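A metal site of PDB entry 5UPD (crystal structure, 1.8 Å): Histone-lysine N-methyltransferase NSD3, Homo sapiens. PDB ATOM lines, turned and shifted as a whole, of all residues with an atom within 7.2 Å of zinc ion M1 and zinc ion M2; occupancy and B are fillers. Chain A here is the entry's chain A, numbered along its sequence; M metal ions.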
ATOM      1  N   ARG A  45      -9.708 -34.756  -9.179  1.00  0.00           N
ATOM      2  CA  ARG A  45     -10.724 -33.849  -8.678  1.00  0.00           C
ATOM      3  C   ARG A  45     -10.861 -34.056  -7.160  1.00  0.00           C
ATOM      4  O   ARG A  45     -10.987 -35.158  -6.699  1.00  0.00           O
ATOM      5  CB  ARG A  45     -12.058 -34.124  -9.385  1.00  0.00           C
ATOM      6  CG  ARG A  45     -13.266 -33.352  -8.858  1.00  0.00           C
ATOM      7  CD  ARG A  45     -14.570 -33.623  -9.630  1.00  0.00           C
ATOM      8  NE  ARG A  45     -14.407 -33.326 -11.061  1.00  0.00           N
ATOM      9  CZ  ARG A  45     -14.433 -34.208 -12.069  1.00  0.00           C
ATOM     10  NH1 ARG A  45     -14.667 -35.513 -11.866  1.00  0.00           N
ATOM     11  NH2 ARG A  45     -14.233 -33.781 -13.317  1.00  0.00           N
ATOM     12  N   CYS A  46     -10.824 -32.975  -6.409  1.00  0.00           N
ATOM     13  CA  CYS A  46     -11.046 -33.010  -4.978  1.00  0.00           C
ATOM     14  C   CYS A  46     -12.571 -32.984  -4.657  1.00  0.00           C
ATOM     15  O   CYS A  46     -13.407 -32.835  -5.551  1.00  0.00           O
ATOM     16  CB  CYS A  46     -10.377 -31.816  -4.354  1.00  0.00           C
ATOM     17  SG  CYS A  46     -11.175 -30.220  -4.659  1.00  0.00           S
ATOM     18  N   ASN A  47     -12.891 -33.038  -3.369  1.00  0.00           N
ATOM     19  CA  ASN A  47     -14.278 -33.102  -2.900  1.00  0.00           C
ATOM     20  C   ASN A  47     -14.723 -31.792  -2.224  1.00  0.00           C
ATOM     21  O   ASN A  47     -15.781 -31.739  -1.605  1.00  0.00           O
ATOM     22  CB  ASN A  47     -14.470 -34.300  -1.930  1.00  0.00           C
ATOM     23  CG  ASN A  47     -14.256 -35.683  -2.607  1.00  0.00           C
ATOM     24  OD1 ASN A  47     -14.342 -35.839  -3.831  1.00  0.00           O
ATOM     25  ND2 ASN A  47     -14.014 -36.708  -1.786  1.00  0.00           N
ATOM     26  N   CYS A  48     -13.920 -30.728  -2.363  1.00  0.00           N
ATOM     27  CA  CYS A  48     -14.257 -29.404  -1.827  1.00  0.00           C
ATOM     28  C   CYS A  48     -15.492 -28.776  -2.511  1.00  0.00           C
ATOM     29  O   CYS A  48     -15.850 -29.158  -3.607  1.00  0.00           O
ATOM     30  CB  CYS A  48     -13.072 -28.438  -1.922  1.00  0.00           C
ATOM     31  SG  CYS A  48     -11.504 -28.990  -1.167  1.00  0.00           S
ATOM     32  N   LYS A  49     -16.110 -27.793  -1.858  1.00  0.00           N
ATOM     33  CA  LYS A  49     -17.383 -27.235  -2.350  1.00  0.00           C
ATOM     34  C   LYS A  49     -17.305 -25.736  -2.527  1.00  0.00           C
ATOM     35  O   LYS A  49     -16.613 -25.035  -1.766  1.00  0.00           O
ATOM     36  CB  LYS A  49     -18.556 -27.635  -1.422  1.00  0.00           C
ATOM     37  CG  LYS A  49     -19.065 -29.048  -1.680  1.00  0.00           C
ATOM     38  CD  LYS A  49     -19.754 -29.671  -0.469  1.00  0.00           C
ATOM     39  CE  LYS A  49     -20.351 -31.031  -0.813  1.00  0.00           C
ATOM     40  NZ  LYS A  49     -21.193 -31.554   0.304  1.00  0.00           N
ATOM     41  N   ASP A  52     -17.846 -23.860   0.635  1.00  0.00           N
ATOM     42  CA  ASP A  52     -16.898 -23.869   1.766  1.00  0.00           C
ATOM     43  C   ASP A  52     -16.303 -22.476   1.879  1.00  0.00           C
ATOM     44  O   ASP A  52     -16.301 -21.720   0.912  1.00  0.00           O
ATOM     45  CB  ASP A  52     -15.755 -24.883   1.564  1.00  0.00           C
ATOM     46  CG  ASP A  52     -16.243 -26.336   1.499  1.00  0.00           C
ATOM     47  OD1 ASP A  52     -17.449 -26.605   1.724  1.00  0.00           O
ATOM     48  OD2 ASP A  52     -15.393 -27.237   1.225  1.00  0.00           O
ATOM     49  N   PRO A  55     -12.196 -22.356  -0.259  1.00  0.00           N
ATOM     50  CA  PRO A  55     -12.164 -23.665  -0.905  1.00  0.00           C
ATOM     51  C   PRO A  55     -10.738 -24.019  -1.458  1.00  0.00           C
ATOM     52  O   PRO A  55     -10.112 -23.192  -2.075  1.00  0.00           O
ATOM     53  CB  PRO A  55     -13.203 -23.544  -2.028  1.00  0.00           C
ATOM     54  CG  PRO A  55     -13.503 -22.091  -2.151  1.00  0.00           C
ATOM     55  CD  PRO A  55     -13.197 -21.448  -0.850  1.00  0.00           C
ATOM     56  N   CYS A  56     -10.307 -25.242  -1.166  1.00  0.00           N
ATOM     57  CA  CYS A  56      -8.980 -25.762  -1.511  1.00  0.00           C
ATOM     58  C   CYS A  56      -7.821 -24.977  -0.894  1.00  0.00           C
ATOM     59  O   CYS A  56      -6.709 -25.060  -1.369  1.00  0.00           O
ATOM     60  CB  CYS A  56      -8.824 -25.920  -3.028  1.00  0.00           C
ATOM     61  SG  CYS A  56     -10.210 -26.833  -3.791  1.00  0.00           S
ATOM     62  N   GLY A  57      -8.076 -24.303   0.227  1.00  0.00           N
ATOM     63  CA  GLY A  57      -7.098 -23.440   0.892  1.00  0.00           C
ATOM     64  C   GLY A  57      -6.186 -24.188   1.847  1.00  0.00           C
ATOM     65  O   GLY A  57      -6.333 -25.400   2.104  1.00  0.00           O
ATOM     66  N   SER A  60      -7.990 -26.168   4.654  1.00  0.00           N
ATOM     67  CA  SER A  60      -8.986 -27.169   4.226  1.00  0.00           C
ATOM     68  C   SER A  60      -8.495 -28.614   4.253  1.00  0.00           C
ATOM     69  O   SER A  60      -7.317 -28.868   4.385  1.00  0.00           O
ATOM     70  CB  SER A  60      -9.451 -26.837   2.803  1.00  0.00           C
ATOM     71  OG  SER A  60      -8.457 -27.163   1.848  1.00  0.00           O
ATOM     72  N   GLU A  61      -9.421 -29.561   4.102  1.00  0.00           N
ATOM     73  CA  GLU A  61      -9.047 -30.962   3.990  1.00  0.00           C
ATOM     74  C   GLU A  61      -8.851 -31.339   2.512  1.00  0.00           C
ATOM     75  O   GLU A  61      -8.976 -32.501   2.163  1.00  0.00           O
ATOM     76  CB  GLU A  61     -10.147 -31.861   4.591  1.00  0.00           C
ATOM     77  N   CYS A  62      -8.528 -30.371   1.636  1.00  0.00           N
ATOM     78  CA  CYS A  62      -8.552 -30.634   0.197  1.00  0.00           C
ATOM     79  C   CYS A  62      -7.682 -31.837  -0.092  1.00  0.00           C
ATOM     80  O   CYS A  62      -6.519 -31.855   0.300  1.00  0.00           O
ATOM     81  CB  CYS A  62      -8.028 -29.430  -0.564  1.00  0.00           C
ATOM     82  SG  CYS A  62      -7.953 -29.683  -2.364  1.00  0.00           S
ATOM     83  N   LEU A  63      -8.261 -32.848  -0.746  1.00  0.00           N
ATOM     84  CA  LEU A  63      -7.527 -34.059  -1.104  1.00  0.00           C
ATOM     85  C   LEU A  63      -6.414 -33.763  -2.087  1.00  0.00           C
ATOM     86  O   LEU A  63      -5.435 -34.454  -2.054  1.00  0.00           O
ATOM     87  CB  LEU A  63      -8.436 -35.131  -1.701  1.00  0.00           C
ATOM     88  CG  LEU A  63      -9.578 -35.726  -0.847  1.00  0.00           C
ATOM     89  CD1 LEU A  63     -10.599 -36.356  -1.771  1.00  0.00           C
ATOM     90  CD2 LEU A  63      -9.074 -36.747   0.189  1.00  0.00           C
ATOM     91  N   ASN A  64      -6.560 -32.763  -2.952  1.00  0.00           N
ATOM     92  CA  ASN A  64      -5.507 -32.462  -3.934  1.00  0.00           C
ATOM     93  C   ASN A  64      -4.332 -31.835  -3.187  1.00  0.00           C
ATOM     94  O   ASN A  64      -3.208 -32.268  -3.344  1.00  0.00           O
ATOM     95  CB  ASN A  64      -5.977 -31.555  -5.071  1.00  0.00           C
ATOM     96  CG  ASN A  64      -6.732 -32.305  -6.153  1.00  0.00           C
ATOM     97  OD1 ASN A  64      -6.754 -33.541  -6.172  1.00  0.00           O
ATOM     98  ND2 ASN A  64      -7.319 -31.570  -7.066  1.00  0.00           N
ATOM     99  N   ARG A  65      -4.585 -30.812  -2.392  1.00  0.00           N
ATOM    100  CA  ARG A  65      -3.534 -30.235  -1.525  1.00  0.00           C
ATOM    101  C   ARG A  65      -2.767 -31.244  -0.741  1.00  0.00           C
ATOM    102  O   ARG A  65      -1.534 -31.105  -0.634  1.00  0.00           O
ATOM    103  CB  ARG A  65      -4.118 -29.333  -0.464  1.00  0.00           C
ATOM    104  CG  ARG A  65      -4.417 -27.961  -0.927  1.00  0.00           C
ATOM    105  CD  ARG A  65      -4.138 -26.976   0.162  1.00  0.00           C
ATOM    106  NE  ARG A  65      -4.150 -25.704  -0.515  1.00  0.00           N
ATOM    107  CZ  ARG A  65      -3.088 -24.966  -0.775  1.00  0.00           C
ATOM    108  NH1 ARG A  65      -1.875 -25.305  -0.379  1.00  0.00           N
ATOM    109  NH2 ARG A  65      -3.273 -23.836  -1.439  1.00  0.00           N
ATOM    110  N   GLU A  70      -1.868 -29.650  -7.654  1.00  0.00           N
ATOM    111  CA  GLU A  70      -2.588 -28.419  -7.966  1.00  0.00           C
ATOM    112  C   GLU A  70      -3.918 -28.758  -8.669  1.00  0.00           C
ATOM    113  O   GLU A  70      -3.968 -29.620  -9.540  1.00  0.00           O
ATOM    114  CB  GLU A  70      -1.716 -27.508  -8.863  1.00  0.00           C
ATOM    115  CG  GLU A  70      -2.382 -26.246  -9.330  1.00  0.00           C
ATOM    116  CD  GLU A  70      -1.475 -24.992  -9.388  1.00  0.00           C
ATOM    117  OE1 GLU A  70      -0.721 -24.735  -8.431  1.00  0.00           O
ATOM    118  OE2 GLU A  70      -1.567 -24.238 -10.395  1.00  0.00           O
ATOM    119  N   CYS A  71      -4.981 -28.070  -8.279  1.00  0.00           N
ATOM    120  CA  CYS A  71      -6.281 -28.153  -8.974  1.00  0.00           C
ATOM    121  C   CYS A  71      -6.203 -27.475 -10.324  1.00  0.00           C
ATOM    122  O   CYS A  71      -5.411 -26.557 -10.549  1.00  0.00           O
ATOM    123  CB  CYS A  71      -7.386 -27.473  -8.131  1.00  0.00           C
ATOM    124  SG  CYS A  71      -7.770 -28.206  -6.561  1.00  0.00           S
ATOM    125  N   HIS A  72      -6.960 -27.981 -11.276  1.00  0.00           N
ATOM    126  CA  HIS A  72      -7.082 -27.367 -12.574  1.00  0.00           C
ATOM    127  C   HIS A  72      -8.462 -26.688 -12.546  1.00  0.00           C
ATOM    128  O   HIS A  72      -9.426 -27.331 -12.163  1.00  0.00           O
ATOM    129  CB  HIS A  72      -7.080 -28.432 -13.659  1.00  0.00           C
ATOM    130  CG  HIS A  72      -7.026 -27.867 -15.036  1.00  0.00           C
ATOM    131  ND1 HIS A  72      -8.069 -27.121 -15.567  1.00  0.00           N
ATOM    132  CD2 HIS A  72      -6.086 -27.970 -16.005  1.00  0.00           C
ATOM    133  CE1 HIS A  72      -7.738 -26.749 -16.795  1.00  0.00           C
ATOM    134  NE2 HIS A  72      -6.546 -27.264 -17.097  1.00  0.00           N
ATOM    135  N   PRO A  73      -8.567 -25.406 -12.960  1.00  0.00           N
ATOM    136  CA  PRO A  73      -9.830 -24.655 -12.859  1.00  0.00           C
ATOM    137  C   PRO A  73     -11.029 -25.303 -13.615  1.00  0.00           C
ATOM    138  O   PRO A  73     -12.145 -25.250 -13.113  1.00  0.00           O
ATOM    139  CB  PRO A  73      -9.471 -23.275 -13.418  1.00  0.00           C
ATOM    140  CG  PRO A  73      -8.283 -23.494 -14.267  1.00  0.00           C
ATOM    141  CD  PRO A  73      -7.511 -24.576 -13.573  1.00  0.00           C
ATOM    142  N   VAL A  75     -11.570 -28.488 -13.759  1.00  0.00           N
ATOM    143  CA  VAL A  75     -11.894 -29.739 -13.081  1.00  0.00           C
ATOM    144  C   VAL A  75     -12.434 -29.483 -11.672  1.00  0.00           C
ATOM    145  O   VAL A  75     -13.306 -30.205 -11.222  1.00  0.00           O
ATOM    146  CB  VAL A  75     -10.641 -30.658 -13.016  1.00  0.00           C
ATOM    147  CG1 VAL A  75     -10.894 -31.933 -12.210  1.00  0.00           C
ATOM    148  CG2 VAL A  75     -10.204 -31.052 -14.416  1.00  0.00           C
ATOM    149  N   CYS A  76     -11.937 -28.471 -10.989  1.00  0.00           N
ATOM    150  CA  CYS A  76     -12.222 -28.303  -9.588  1.00  0.00           C
ATOM    151  C   CYS A  76     -13.676 -27.949  -9.363  1.00  0.00           C
ATOM    152  O   CYS A  76     -14.172 -27.035 -10.016  1.00  0.00           O
ATOM    153  CB  CYS A  76     -11.383 -27.177  -8.995  1.00  0.00           C
ATOM    154  SG  CYS A  76     -11.573 -27.106  -7.234  1.00  0.00           S
ATOM    155  N   PRO A  77     -14.343 -28.611  -8.391  1.00  0.00           N
ATOM    156  CA  PRO A  77     -15.733 -28.257  -8.109  1.00  0.00           C
ATOM    157  C   PRO A  77     -15.910 -26.844  -7.552  1.00  0.00           C
ATOM    158  O   PRO A  77     -17.004 -26.274  -7.706  1.00  0.00           O
ATOM    159  CB  PRO A  77     -16.190 -29.304  -7.073  1.00  0.00           C
ATOM    160  CG  PRO A  77     -15.150 -30.378  -7.118  1.00  0.00           C
ATOM    161  CD  PRO A  77     -13.894 -29.678  -7.480  1.00  0.00           C
ATOM    162  N   ALA A  78     -14.859 -26.264  -6.950  1.00  0.00           N
ATOM    163  CA  ALA A  78     -14.924 -24.865  -6.527  1.00  0.00           C
ATOM    164  C   ALA A  78     -14.665 -23.862  -7.649  1.00  0.00           C
ATOM    165  O   ALA A  78     -14.678 -22.656  -7.418  1.00  0.00           O
ATOM    166  CB  ALA A  78     -13.967 -24.617  -5.368  1.00  0.00           C
ATOM    167  N   GLY A  79     -14.385 -24.340  -8.860  1.00  0.00           N
ATOM    168  CA  GLY A  79     -14.164 -23.464  -9.998  1.00  0.00           C
ATOM    169  C   GLY A  79     -13.058 -22.442  -9.741  1.00  0.00           C
ATOM    170  O   GLY A  79     -11.904 -22.814  -9.564  1.00  0.00           O
ATOM    171  N   ARG A  81     -13.107 -19.921  -7.317  1.00  0.00           N
ATOM    172  CA  ARG A  81     -12.826 -19.681  -5.902  1.00  0.00           C
ATOM    173  C   ARG A  81     -11.775 -20.652  -5.331  1.00  0.00           C
ATOM    174  O   ARG A  81     -11.402 -20.536  -4.187  1.00  0.00           O
ATOM    175  CB  ARG A  81     -14.109 -19.786  -5.052  1.00  0.00           C
ATOM    176  CG  ARG A  81     -15.229 -18.845  -5.485  1.00  0.00           C
ATOM    177  CD  ARG A  81     -16.010 -18.243  -4.319  1.00  0.00           C
ATOM    178  NE  ARG A  81     -16.355 -19.208  -3.254  1.00  0.00           N
ATOM    179  CZ  ARG A  81     -15.865 -19.208  -2.000  1.00  0.00           C
ATOM    180  NH1 ARG A  81     -16.282 -20.126  -1.124  1.00  0.00           N
ATOM    181  NH2 ARG A  81     -14.961 -18.299  -1.588  1.00  0.00           N
ATOM    182  N   CYS A  82     -11.348 -21.622  -6.141  1.00  0.00           N
ATOM    183  CA  CYS A  82     -10.349 -22.593  -5.725  1.00  0.00           C
ATOM    184  C   CYS A  82      -9.060 -21.864  -5.305  1.00  0.00           C
ATOM    185  O   CYS A  82      -8.502 -21.129  -6.111  1.00  0.00           O
ATOM    186  CB  CYS A  82     -10.057 -23.543  -6.888  1.00  0.00           C
ATOM    187  SG  CYS A  82      -8.698 -24.725  -6.608  1.00  0.00           S
ATOM    188  N   GLN A  83      -8.587 -22.105  -4.093  1.00  0.00           N
ATOM    189  CA  GLN A  83      -7.339 -21.502  -3.586  1.00  0.00           C
ATOM    190  C   GLN A  83      -6.119 -22.444  -3.752  1.00  0.00           C
ATOM    191  O   GLN A  83      -5.129 -22.295  -3.041  1.00  0.00           O
ATOM    192  CB  GLN A  83      -7.509 -21.078  -2.118  1.00  0.00           C
ATOM    193  CG  GLN A  83      -8.435 -19.870  -1.955  1.00  0.00           C
ATOM    194  CD  GLN A  83      -8.817 -19.608  -0.499  1.00  0.00           C
ATOM    195  OE1 GLN A  83      -8.289 -20.245   0.433  1.00  0.00           O
ATOM    196  NE2 GLN A  83      -9.760 -18.664  -0.295  1.00  0.00           N
ATOM    197  N   ASN A  84      -6.196 -23.376  -4.721  1.00  0.00           N
ATOM    198  CA  ASN A  84      -5.112 -24.344  -4.969  1.00  0.00           C
ATOM    199  C   ASN A  84      -4.680 -24.229  -6.386  1.00  0.00           C
ATOM    200  O   ASN A  84      -4.587 -25.223  -7.075  1.00  0.00           O
ATOM    201  CB  ASN A  84      -5.526 -25.747  -4.594  1.00  0.00           C
ATOM    202  CG  ASN A  84      -4.377 -26.778  -4.654  1.00  0.00           C
ATOM    203  OD1 ASN A  84      -3.182 -26.438  -4.511  1.00  0.00           O
ATOM    204  ND2 ASN A  84      -4.742 -28.009  -4.891  1.00  0.00           N
ATOM    205  N   GLN A  85      -4.409 -23.001  -6.815  1.00  0.00           N
ATOM    206  CA  GLN A  85      -3.925 -22.748  -8.179  1.00  0.00           C
ATOM    207  C   GLN A  85      -2.664 -21.901  -8.176  1.00  0.00           C
ATOM    208  O   GLN A  85      -2.424 -21.145  -9.117  1.00  0.00           O
ATOM    209  CB  GLN A  85      -4.967 -21.993  -8.984  1.00  0.00           C
ATOM    210  CG  GLN A  85      -6.274 -22.784  -9.187  1.00  0.00           C
ATOM    211  CD  GLN A  85      -7.313 -21.923  -9.888  1.00  0.00           C
ATOM    212  OE1 GLN A  85      -7.198 -21.670 -11.072  1.00  0.00           O
ATOM    213  NE2 GLN A  85      -8.311 -21.439  -9.135  1.00  0.00           N
HETATM  214 ZN    ZN M   1     -10.097 -28.920  -3.055  1.00  0.00          ZN
HETATM  215 ZN    ZN M   2      -9.540 -26.736  -6.062  1.00  0.00          ZN
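The backbone carbonyl oxygen (O) of Cys 56 is in hydrogen-bond range of the guanidinium group (NE) of Arg 65, 2.8 Å away.
The backbone NH of Asn 84 lies close to the side-chain sulfur of Cys 82, at 3.4 Å.
The backbone carbonyl oxygen of Cys 82 is in hydrogen-bond range of the side-chain amide nitrogen of Gln 85 (3.0 Å).
N of Cys 71 is in hydrogen-bond range of O of Asn 84, at 3.1 Å.
SG of Cys 76 lies close to N of Ala 78.
SG of Cys 62 sits close to N of Asn 64, 3.4 Å away.
N of Cys 62 sits close to OG of Ser 60, at 3.2 Å.
The side-chain sulfur of Cys 62 lies close to the backbone NH of Arg 65 (3.6 Å).
Within 4 Å of zinc ion M2: Cys 56, Cys 71, Cys 76 and Cys 82.
The nearest printed residue that does not touch zinc ion M2 is Cys 46 (4.1 Å).
Zinc ion M1 is bound by SG of Cys 56 (2.2 Å).
Zinc ion M1 is bound by the side-chain sulfur (SG) of Cys 46 (2.3 Å).
SG of Cys 48 binds zinc ion M1, 2.4 Å away.
SG of Cys 62 is bound to zinc ion M1 (2.4 Å).
Zinc ion M2 is bound by the side-chain sulfur (SG) of Cys 82 (2.2 Å), the side-chain sulfur (SG) of Cys 71 (2.4 Å), the side-chain sulfur (SG) of Cys 56 (2.4 Å) and the side-chain sulfur (SG) of Cys 76 (2.4 Å).
Of the 29 residues printed, 4 come within 4 Å of zinc ion M1.
The nearest printed residue that does not touch zinc ion M1 is Cys 71 (4.3 Å).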
